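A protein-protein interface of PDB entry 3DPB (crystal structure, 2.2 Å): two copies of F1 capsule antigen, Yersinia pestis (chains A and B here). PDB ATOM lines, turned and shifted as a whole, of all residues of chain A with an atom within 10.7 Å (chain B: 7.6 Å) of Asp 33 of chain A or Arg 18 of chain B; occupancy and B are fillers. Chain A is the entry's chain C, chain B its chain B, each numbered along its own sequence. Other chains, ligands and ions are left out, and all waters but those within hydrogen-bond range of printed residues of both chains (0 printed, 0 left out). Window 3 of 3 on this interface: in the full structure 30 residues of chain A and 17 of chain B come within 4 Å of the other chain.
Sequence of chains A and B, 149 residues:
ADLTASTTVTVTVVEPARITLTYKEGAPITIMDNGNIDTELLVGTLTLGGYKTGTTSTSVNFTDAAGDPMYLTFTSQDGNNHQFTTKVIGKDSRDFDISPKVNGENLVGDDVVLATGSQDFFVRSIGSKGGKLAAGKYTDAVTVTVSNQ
Printed residues of chain A that touch a printed residue of chain B: Ile 29, Thr 30, Ile 31, Met 32, Asp 33, Leu 133 and Ala 135.
Hydrophobic or aromatic side chains of chain A within 4 Å of the printed part of chain B: Ile 31 and Ala 135.
Of the 15 printed residues of chain B, 4 touch a printed residue of chain A.
Hydrophobic or aromatic side chains of chain B that line the printed part of chain A: Val 14 and Pro 16.
Among the printed residues, 12 pairs touch across the chains.
Among the printed residues, no Asp or Glu carboxylate lies within 4 Å of a Lys or Arg side-chain nitrogen of the other chain.
No position is printed for both chains.
Of the 12 pairs that touch across the chains among the printed residues, none has its exchanged pair printed and touching as well.
The backbone NH (N) of Val 14 of chain B is in hydrogen-bond range of the backbone carbonyl oxygen (O) of Ile 29 of chain A (2.6 Å).
The side-chain carboxylate (OE2) of Glu 15 of chain B sits at hydrogen-bond distance from the backbone NH (N) of Ala 135 of chain A, 3.0 Å away.
O of Ile 31 of chain A sits at hydrogen-bond distance from NH2 of Arg 18 of chain B (2.9 Å).
The backbone NH (N) of Ile 31 of chain A is in hydrogen-bond range of the backbone carbonyl oxygen (O) of Val 14 of chain B (2.8 Å).
Asp 33 of chain A touches just one residue of chain B: Arg 18 (3.6 Å).
Printed residues of chain A within 4 Å of Arg 18 of chain B: Ile 31 (2.9 Å), Met 32 (3.4 Å) and Asp 33 (3.6 Å).
Pro 16 of chain B touches just these residues of chain A: Thr 30 and Ile 31.
No residue of chain A comes within 4 Å of Ala 17 of chain B.
No residue of chain A comes within 4 Å of Ile 19 of chain B.
No residue of chain A comes within 4 Å of Gly 50 of chain B.
Of the printed residues of chain B, Met 32 of chain A touches Arg 18.
Of the printed residues of chain B, Leu 133 of chain A touches Glu 15.
Of the printed residues of chain B, Ile 29 of chain A touches Val 14.
Of the printed residues of chain A, Glu 15 of chain B touches Ile 31, Leu 133 and Ala 135.
Of the printed residues of chain B, Thr 30 of chain A touches Val 14 (3.4 Å) and Pro 16 (3.3 Å).
The nearest residue of chain A that does not touch Arg 18 of chain B is Thr 30 of chain A (4.3 Å).
The nearest printed residue of chain A that does not touch Val 14 of chain B is Met 32 of chain A (6.0 Å).
Thr 30 of chain A touches Val 14 of chain B.
Thr 30 of chain A touches Pro 16 of chain B.
Ile 31 of chain A touches Glu 15 of chain B (CG1 to CG, 3.98 Å).
Pro 16 of chain B touches Ile 31 of chain A.
CA of Met 32 of chain A touches NH2 of Arg 18 of chain B (3.4 Å).
Arg 18 of chain B touches Asp 33 of chain A.
Leu 133 of chain A touches Glu 15 of chain B (O to OE2, 3.9 Å).
Ala 135 of chain A touches Val 14 of chain B.
The backbone carbonyl oxygen (O) of Arg 18 of chain B lies within hydrogen-bond range of the backbone NH (N) of Tyr 51 of chain B, at 3.4 Å.
The backbone NH (N) of Leu 133 of chain A lies within hydrogen-bond range of the backbone carbonyl oxygen (O) of Gly 35 of chain A (2.9 Å).
NZ of Lys 52 of chain B is in salt-bridge range of OE1 of Glu 15 of chain B (2.4 Å).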
ATOM      1  N   ILE A  29      15.896 -13.633   1.748  1.00  0.00           N
ATOM      2  CA  ILE A  29      16.003 -14.988   2.277  1.00  0.00           C
ATOM      3  C   ILE A  29      15.996 -14.886   3.800  1.00  0.00           C
ATOM      4  O   ILE A  29      16.740 -14.097   4.375  1.00  0.00           O
ATOM      5  CB  ILE A  29      17.302 -15.743   1.828  1.00  0.00           C
ATOM      6  CG1 ILE A  29      17.525 -15.789   0.298  1.00  0.00           C
ATOM      7  CG2 ILE A  29      17.310 -17.144   2.352  1.00  0.00           C
ATOM      8  CD1 ILE A  29      16.263 -15.689  -0.554  1.00  0.00           C
ATOM      9  N   THR A  30      15.153 -15.677   4.454  1.00  0.00           N
ATOM     10  CA  THR A  30      15.087 -15.667   5.927  1.00  0.00           C
ATOM     11  C   THR A  30      15.940 -16.813   6.437  1.00  0.00           C
ATOM     12  O   THR A  30      15.733 -17.937   6.010  1.00  0.00           O
ATOM     13  CB  THR A  30      13.633 -15.798   6.420  1.00  0.00           C
ATOM     14  OG1 THR A  30      12.918 -14.594   6.117  1.00  0.00           O
ATOM     15  CG2 THR A  30      13.574 -16.014   7.924  1.00  0.00           C
ATOM     16  N   ILE A  31      16.914 -16.516   7.306  1.00  0.00           N
ATOM     17  CA  ILE A  31      17.716 -17.534   7.988  1.00  0.00           C
ATOM     18  C   ILE A  31      16.810 -18.313   8.950  1.00  0.00           C
ATOM     19  O   ILE A  31      16.003 -17.717   9.652  1.00  0.00           O
ATOM     20  CB  ILE A  31      18.854 -16.904   8.857  1.00  0.00           C
ATOM     21  CG1 ILE A  31      19.614 -15.770   8.111  1.00  0.00           C
ATOM     22  CG2 ILE A  31      19.772 -17.994   9.404  1.00  0.00           C
ATOM     23  CD1 ILE A  31      21.033 -16.017   7.826  1.00  0.00           C
ATOM     24  N   MET A  32      16.936 -19.634   8.967  1.00  0.00           N
ATOM     25  CA  MET A  32      16.157 -20.477   9.874  1.00  0.00           C
ATOM     26  C   MET A  32      16.834 -20.591  11.244  1.00  0.00           C
ATOM     27  O   MET A  32      17.982 -20.175  11.393  1.00  0.00           O
ATOM     28  CB  MET A  32      15.986 -21.849   9.269  1.00  0.00           C
ATOM     29  CG  MET A  32      15.227 -21.803   7.973  1.00  0.00           C
ATOM     30  SD  MET A  32      15.249 -23.451   7.266  1.00  0.00           S
ATOM     31  CE  MET A  32      13.492 -23.555   6.921  1.00  0.00           C
ATOM     32  N   ASP A  33      16.148 -21.175  12.235  1.00  0.00           N
ATOM     33  CA  ASP A  33      16.735 -21.229  13.584  1.00  0.00           C
ATOM     34  C   ASP A  33      18.049 -22.012  13.612  1.00  0.00           C
ATOM     35  O   ASP A  33      18.928 -21.720  14.419  1.00  0.00           O
ATOM     36  CB  ASP A  33      15.751 -21.717  14.658  1.00  0.00           C
ATOM     37  CG  ASP A  33      16.190 -21.294  16.079  1.00  0.00           C
ATOM     38  OD1 ASP A  33      16.923 -22.081  16.744  1.00  0.00           O
ATOM     39  OD2 ASP A  33      15.847 -20.152  16.518  1.00  0.00           O
ATOM     40  N   ASN A  34      18.218 -22.965  12.706  1.00  0.00           N
ATOM     41  CA  ASN A  34      19.487 -23.681  12.635  1.00  0.00           C
ATOM     42  C   ASN A  34      20.620 -22.989  11.816  1.00  0.00           C
ATOM     43  O   ASN A  34      21.680 -23.594  11.573  1.00  0.00           O
ATOM     44  CB  ASN A  34      19.237 -25.093  12.134  1.00  0.00           C
ATOM     45  CG  ASN A  34      18.687 -25.116  10.717  1.00  0.00           C
ATOM     46  OD1 ASN A  34      18.579 -24.077  10.043  1.00  0.00           O
ATOM     47  ND2 ASN A  34      18.346 -26.309  10.249  1.00  0.00           N
ATOM     48  N   GLY A  35      20.420 -21.727  11.413  1.00  0.00           N
ATOM     49  CA  GLY A  35      21.448 -21.003  10.620  1.00  0.00           C
ATOM     50  C   GLY A  35      21.486 -21.360   9.126  1.00  0.00           C
ATOM     51  O   GLY A  35      22.328 -20.851   8.365  1.00  0.00           O
ATOM     52  N   ASN A  36      20.567 -22.226   8.698  1.00  0.00           N
ATOM     53  CA  ASN A  36      20.503 -22.652   7.289  1.00  0.00           C
ATOM     54  C   ASN A  36      19.350 -21.948   6.624  1.00  0.00           C
ATOM     55  O   ASN A  36      18.712 -21.111   7.251  1.00  0.00           O
ATOM     56  CB  ASN A  36      20.334 -24.173   7.168  1.00  0.00           C
ATOM     57  CG  ASN A  36      21.056 -24.765   5.940  1.00  0.00           C
ATOM     58  OD1 ASN A  36      21.304 -24.088   4.933  1.00  0.00           O
ATOM     59  ND2 ASN A  36      21.414 -26.035   6.047  1.00  0.00           N
ATOM     60  N   ILE A  37      19.111 -22.245   5.346  1.00  0.00           N
ATOM     61  CA  ILE A  37      18.015 -21.649   4.617  1.00  0.00           C
ATOM     62  C   ILE A  37      17.207 -22.781   4.052  1.00  0.00           C
ATOM     63  O   ILE A  37      17.682 -23.910   3.955  1.00  0.00           O
ATOM     64  CB  ILE A  37      18.474 -20.703   3.456  1.00  0.00           C
ATOM     65  CG1 ILE A  37      19.402 -21.441   2.457  1.00  0.00           C
ATOM     66  CG2 ILE A  37      19.066 -19.418   4.011  1.00  0.00           C
ATOM     67  CD1 ILE A  37      19.860 -20.574   1.301  1.00  0.00           C
ATOM     68  N   ASP A  38      15.994 -22.478   3.641  1.00  0.00           N
ATOM     69  CA  ASP A  38      15.137 -23.488   3.082  1.00  0.00           C
ATOM     70  C   ASP A  38      15.555 -23.661   1.593  1.00  0.00           C
ATOM     71  O   ASP A  38      16.166 -22.752   0.988  1.00  0.00           O
ATOM     72  CB  ASP A  38      13.712 -22.976   3.234  1.00  0.00           C
ATOM     73  CG  ASP A  38      12.664 -24.054   3.165  1.00  0.00           C
ATOM     74  OD1 ASP A  38      12.974 -25.280   3.268  1.00  0.00           O
ATOM     75  OD2 ASP A  38      11.491 -23.629   2.998  1.00  0.00           O
ATOM     76  N   LEU A  41      13.469 -21.921  -2.549  1.00  0.00           N
ATOM     77  CA  LEU A  41      13.027 -20.520  -2.526  1.00  0.00           C
ATOM     78  C   LEU A  41      13.359 -19.780  -3.823  1.00  0.00           C
ATOM     79  O   LEU A  41      14.411 -19.969  -4.380  1.00  0.00           O
ATOM     80  CB  LEU A  41      13.688 -19.767  -1.385  1.00  0.00           C
ATOM     81  CG  LEU A  41      13.552 -20.421  -0.018  1.00  0.00           C
ATOM     82  CD1 LEU A  41      14.589 -19.789   0.872  1.00  0.00           C
ATOM     83  CD2 LEU A  41      12.100 -20.308   0.549  1.00  0.00           C
ATOM     84  N   GLY A 131      28.156 -24.615   7.771  1.00  0.00           N
ATOM     85  CA  GLY A 131      28.014 -23.787   8.967  1.00  0.00           C
ATOM     86  C   GLY A 131      26.852 -22.811   8.834  1.00  0.00           C
ATOM     87  O   GLY A 131      26.231 -22.709   7.772  1.00  0.00           O
ATOM     88  N   LYS A 132      26.574 -22.091   9.910  1.00  0.00           N
ATOM     89  CA  LYS A 132      25.474 -21.141   9.970  1.00  0.00           C
ATOM     90  C   LYS A 132      25.791 -19.909   9.121  1.00  0.00           C
ATOM     91  O   LYS A 132      26.912 -19.457   9.099  1.00  0.00           O
ATOM     92  CB  LYS A 132      25.229 -20.710  11.430  1.00  0.00           C
ATOM     93  CG  LYS A 132      24.976 -21.868  12.430  1.00  0.00           C
ATOM     94  CD  LYS A 132      24.657 -21.337  13.832  1.00  0.00           C
ATOM     95  CE  LYS A 132      23.125 -21.312  14.113  1.00  0.00           C
ATOM     96  NZ  LYS A 132      22.756 -20.679  15.453  1.00  0.00           N
ATOM     97  N   LEU A 133      24.793 -19.355   8.458  1.00  0.00           N
ATOM     98  CA  LEU A 133      24.990 -18.147   7.656  1.00  0.00           C
ATOM     99  C   LEU A 133      24.789 -16.914   8.538  1.00  0.00           C
ATOM    100  O   LEU A 133      24.004 -16.943   9.491  1.00  0.00           O
ATOM    101  CB  LEU A 133      24.037 -18.125   6.468  1.00  0.00           C
ATOM    102  CG  LEU A 133      24.098 -19.208   5.382  1.00  0.00           C
ATOM    103  CD1 LEU A 133      22.832 -19.140   4.504  1.00  0.00           C
ATOM    104  CD2 LEU A 133      25.414 -19.157   4.520  1.00  0.00           C
ATOM    105  N   ALA A 135      23.337 -13.145   8.454  1.00  0.00           N
ATOM    106  CA  ALA A 135      22.547 -12.229   7.647  1.00  0.00           C
ATOM    107  C   ALA A 135      23.385 -11.084   7.034  1.00  0.00           C
ATOM    108  O   ALA A 135      24.321 -10.559   7.663  1.00  0.00           O
ATOM    109  CB  ALA A 135      21.389 -11.655   8.467  1.00  0.00           C
ATOM    110  N   VAL B  14      18.196 -12.326   5.572  1.00  0.00           N
ATOM    111  CA  VAL B  14      17.788 -11.678   6.823  1.00  0.00           C
ATOM    112  C   VAL B  14      17.645 -12.644   7.988  1.00  0.00           C
ATOM    113  O   VAL B  14      17.273 -13.797   7.830  1.00  0.00           O
ATOM    114  CB  VAL B  14      16.491 -10.806   6.687  1.00  0.00           C
ATOM    115  CG1 VAL B  14      16.604  -9.838   5.527  1.00  0.00           C
ATOM    116  CG2 VAL B  14      15.255 -11.667   6.549  1.00  0.00           C
ATOM    117  N   GLU B  15      17.977 -12.136   9.165  1.00  0.00           N
ATOM    118  CA  GLU B  15      17.772 -12.837  10.426  1.00  0.00           C
ATOM    119  C   GLU B  15      16.502 -12.293  11.086  1.00  0.00           C
ATOM    120  O   GLU B  15      16.384 -11.071  11.332  1.00  0.00           O
ATOM    121  CB  GLU B  15      18.950 -12.643  11.390  1.00  0.00           C
ATOM    122  CG  GLU B  15      19.791 -13.911  11.625  1.00  0.00           C
ATOM    123  CD  GLU B  15      21.262 -13.593  11.964  1.00  0.00           C
ATOM    124  OE1 GLU B  15      21.462 -12.999  13.055  1.00  0.00           O
ATOM    125  OE2 GLU B  15      22.213 -13.917  11.171  1.00  0.00           O
ATOM    126  N   PRO B  16      15.551 -13.180  11.374  1.00  0.00           N
ATOM    127  CA  PRO B  16      14.353 -12.742  12.084  1.00  0.00           C
ATOM    128  C   PRO B  16      14.590 -12.616  13.571  1.00  0.00           C
ATOM    129  O   PRO B  16      15.612 -13.078  14.058  1.00  0.00           O
ATOM    130  CB  PRO B  16      13.354 -13.872  11.838  1.00  0.00           C
ATOM    131  CG  PRO B  16      13.987 -14.854  10.953  1.00  0.00           C
ATOM    132  CD  PRO B  16      15.493 -14.606  11.018  1.00  0.00           C
ATOM    133  N   ALA B  17      13.636 -11.997  14.277  1.00  0.00           N
ATOM    134  CA  ALA B  17      13.644 -11.846  15.729  1.00  0.00           C
ATOM    135  C   ALA B  17      12.671 -12.840  16.339  1.00  0.00           C
ATOM    136  O   ALA B  17      11.499 -12.550  16.450  1.00  0.00           O
ATOM    137  CB  ALA B  17      13.247 -10.444  16.092  1.00  0.00           C
ATOM    138  N   ARG B  18      13.185 -14.004  16.710  1.00  0.00           N
ATOM    139  CA  ARG B  18      12.439 -15.094  17.294  1.00  0.00           C
ATOM    140  C   ARG B  18      12.582 -15.088  18.799  1.00  0.00           C
ATOM    141  O   ARG B  18      13.704 -14.984  19.309  1.00  0.00           O
ATOM    142  CB  ARG B  18      13.010 -16.427  16.801  1.00  0.00           C
ATOM    143  CG  ARG B  18      12.984 -16.633  15.336  1.00  0.00           C
ATOM    144  CD  ARG B  18      13.206 -18.108  15.032  1.00  0.00           C
ATOM    145  NE  ARG B  18      13.092 -18.390  13.596  1.00  0.00           N
ATOM    146  CZ  ARG B  18      14.088 -18.217  12.726  1.00  0.00           C
ATOM    147  NH1 ARG B  18      15.272 -17.756  13.139  1.00  0.00           N
ATOM    148  NH2 ARG B  18      13.908 -18.507  11.452  1.00  0.00           N
ATOM    149  N   ILE B  19      11.468 -15.186  19.522  1.00  0.00           N
ATOM    150  CA  ILE B  19      11.504 -15.178  20.998  1.00  0.00           C
ATOM    151  C   ILE B  19      10.547 -16.232  21.472  1.00  0.00           C
ATOM    152  O   ILE B  19       9.388 -16.208  21.096  1.00  0.00           O
ATOM    153  CB  ILE B  19      11.070 -13.818  21.622  1.00  0.00           C
ATOM    154  CG1 ILE B  19      12.049 -12.659  21.275  1.00  0.00           C
ATOM    155  CG2 ILE B  19      10.868 -13.966  23.151  1.00  0.00           C
ATOM    156  CD1 ILE B  19      13.547 -12.789  21.856  1.00  0.00           C
ATOM    157  N   THR B  20      11.052 -17.180  22.260  1.00  0.00           N
ATOM    158  CA  THR B  20      10.232 -18.222  22.854  1.00  0.00           C
ATOM    159  C   THR B  20      10.337 -18.211  24.382  1.00  0.00           C
ATOM    160  O   THR B  20      11.293 -17.676  24.959  1.00  0.00           O
ATOM    161  CB  THR B  20      10.628 -19.631  22.354  1.00  0.00           C
ATOM    162  OG1 THR B  20      11.917 -19.954  22.867  1.00  0.00           O
ATOM    163  CG2 THR B  20      10.654 -19.712  20.793  1.00  0.00           C
ATOM    164  N   LEU B  48      13.831 -18.767  28.588  1.00  0.00           N
ATOM    165  CA  LEU B  48      13.750 -17.831  27.489  1.00  0.00           C
ATOM    166  C   LEU B  48      14.620 -18.385  26.379  1.00  0.00           C
ATOM    167  O   LEU B  48      15.737 -18.768  26.632  1.00  0.00           O
ATOM    168  CB  LEU B  48      14.263 -16.449  27.932  1.00  0.00           C
ATOM    169  CG  LEU B  48      14.166 -15.274  26.957  1.00  0.00           C
ATOM    170  CD1 LEU B  48      12.700 -14.888  26.761  1.00  0.00           C
ATOM    171  CD2 LEU B  48      14.919 -14.098  27.489  1.00  0.00           C
ATOM    172  N   GLY B  49      14.088 -18.445  25.164  1.00  0.00           N
ATOM    173  CA  GLY B  49      14.882 -18.863  23.980  1.00  0.00           C
ATOM    174  C   GLY B  49      14.679 -17.961  22.769  1.00  0.00           C
ATOM    175  O   GLY B  49      13.963 -16.928  22.837  1.00  0.00           O
ATOM    176  N   GLY B  50      15.311 -18.356  21.657  1.00  0.00           N
ATOM    177  CA  GLY B  50      15.062 -17.777  20.340  1.00  0.00           C
ATOM    178  C   GLY B  50      15.993 -16.637  20.032  1.00  0.00           C
ATOM    179  O   GLY B  50      16.337 -16.399  18.874  1.00  0.00           O
ATOM    180  N   TYR B  51      16.437 -15.948  21.078  1.00  0.00           N
ATOM    181  CA  TYR B  51      17.197 -14.705  20.926  1.00  0.00           C
ATOM    182  C   TYR B  51      18.610 -14.903  20.342  1.00  0.00           C
ATOM    183  O   TYR B  51      19.187 -16.015  20.382  1.00  0.00           O
ATOM    184  CB  TYR B  51      17.262 -13.937  22.251  1.00  0.00           C
ATOM    185  CG  TYR B  51      17.881 -14.735  23.367  1.00  0.00           C
ATOM    186  CD1 TYR B  51      19.271 -14.885  23.468  1.00  0.00           C
ATOM    187  CD2 TYR B  51      17.090 -15.306  24.348  1.00  0.00           C
ATOM    188  CE1 TYR B  51      19.857 -15.624  24.512  1.00  0.00           C
ATOM    189  CE2 TYR B  51      17.655 -16.052  25.384  1.00  0.00           C
ATOM    190  CZ  TYR B  51      19.025 -16.203  25.460  1.00  0.00           C
ATOM    191  OH  TYR B  51      19.547 -16.952  26.480  1.00  0.00           O
ATOM    192  N   LYS B  52      19.142 -13.814  19.789  1.00  0.00           N
ATOM    193  CA  LYS B  52      20.441 -13.833  19.178  1.00  0.00           C
ATOM    194  C   LYS B  52      21.520 -13.750  20.272  1.00  0.00           C
ATOM    195  O   LYS B  52      21.388 -12.957  21.237  1.00  0.00           O
ATOM    196  CB  LYS B  52      20.581 -12.652  18.208  1.00  0.00           C
ATOM    197  CG  LYS B  52      21.702 -12.830  17.222  1.00  0.00           C
ATOM    198  CD  LYS B  52      21.905 -11.554  16.387  1.00  0.00           C
ATOM    199  CE  LYS B  52      23.133 -11.645  15.455  1.00  0.00           C
ATOM    200  NZ  LYS B  52      23.233 -12.943  14.723  1.00  0.00           N
ATOM    201  N   GLY B 117      21.804 -19.705  23.112  1.00  0.00           N
ATOM    202  CA  GLY B 117      20.679 -20.584  22.867  1.00  0.00           C
ATOM    203  C   GLY B 117      19.466 -20.226  23.730  1.00  0.00           C
ATOM    204  O   GLY B 117      18.476 -19.689  23.221  1.00  0.00           O
ATOM    205  N   VAL B 146      11.291  -8.419  25.519  1.00  0.00           N
ATOM    206  CA  VAL B 146      12.675  -8.519  25.111  1.00  0.00           C
ATOM    207  C   VAL B 146      12.960  -7.474  24.048  1.00  0.00           C
ATOM    208  O   VAL B 146      12.352  -7.491  22.981  1.00  0.00           O
ATOM    209  CB  VAL B 146      13.003  -9.899  24.540  1.00  0.00           C
ATOM    210  CG1 VAL B 146      14.486  -9.929  24.166  1.00  0.00           C
ATOM    211  CG2 VAL B 146      12.652 -10.983  25.549  1.00  0.00           C
ATOM    212  N   ASN B 148      15.321  -6.476  21.437  1.00  0.00           N
ATOM    213  CA  ASN B 148      16.396  -7.105  20.666  1.00  0.00           C
ATOM    214  C   ASN B 148      17.492  -6.078  20.306  1.00  0.00           C
ATOM    215  O   ASN B 148      17.171  -4.931  19.975  1.00  0.00           O
ATOM    216  CB  ASN B 148      15.836  -7.790  19.431  1.00  0.00           C
ATOM    217  CG  ASN B 148      14.938  -8.990  19.773  1.00  0.00           C
ATOM    218  OD1 ASN B 148      15.424 -10.091  19.988  1.00  0.00           O
ATOM    219  ND2 ASN B 148      13.617  -8.779  19.790  1.00  0.00           N
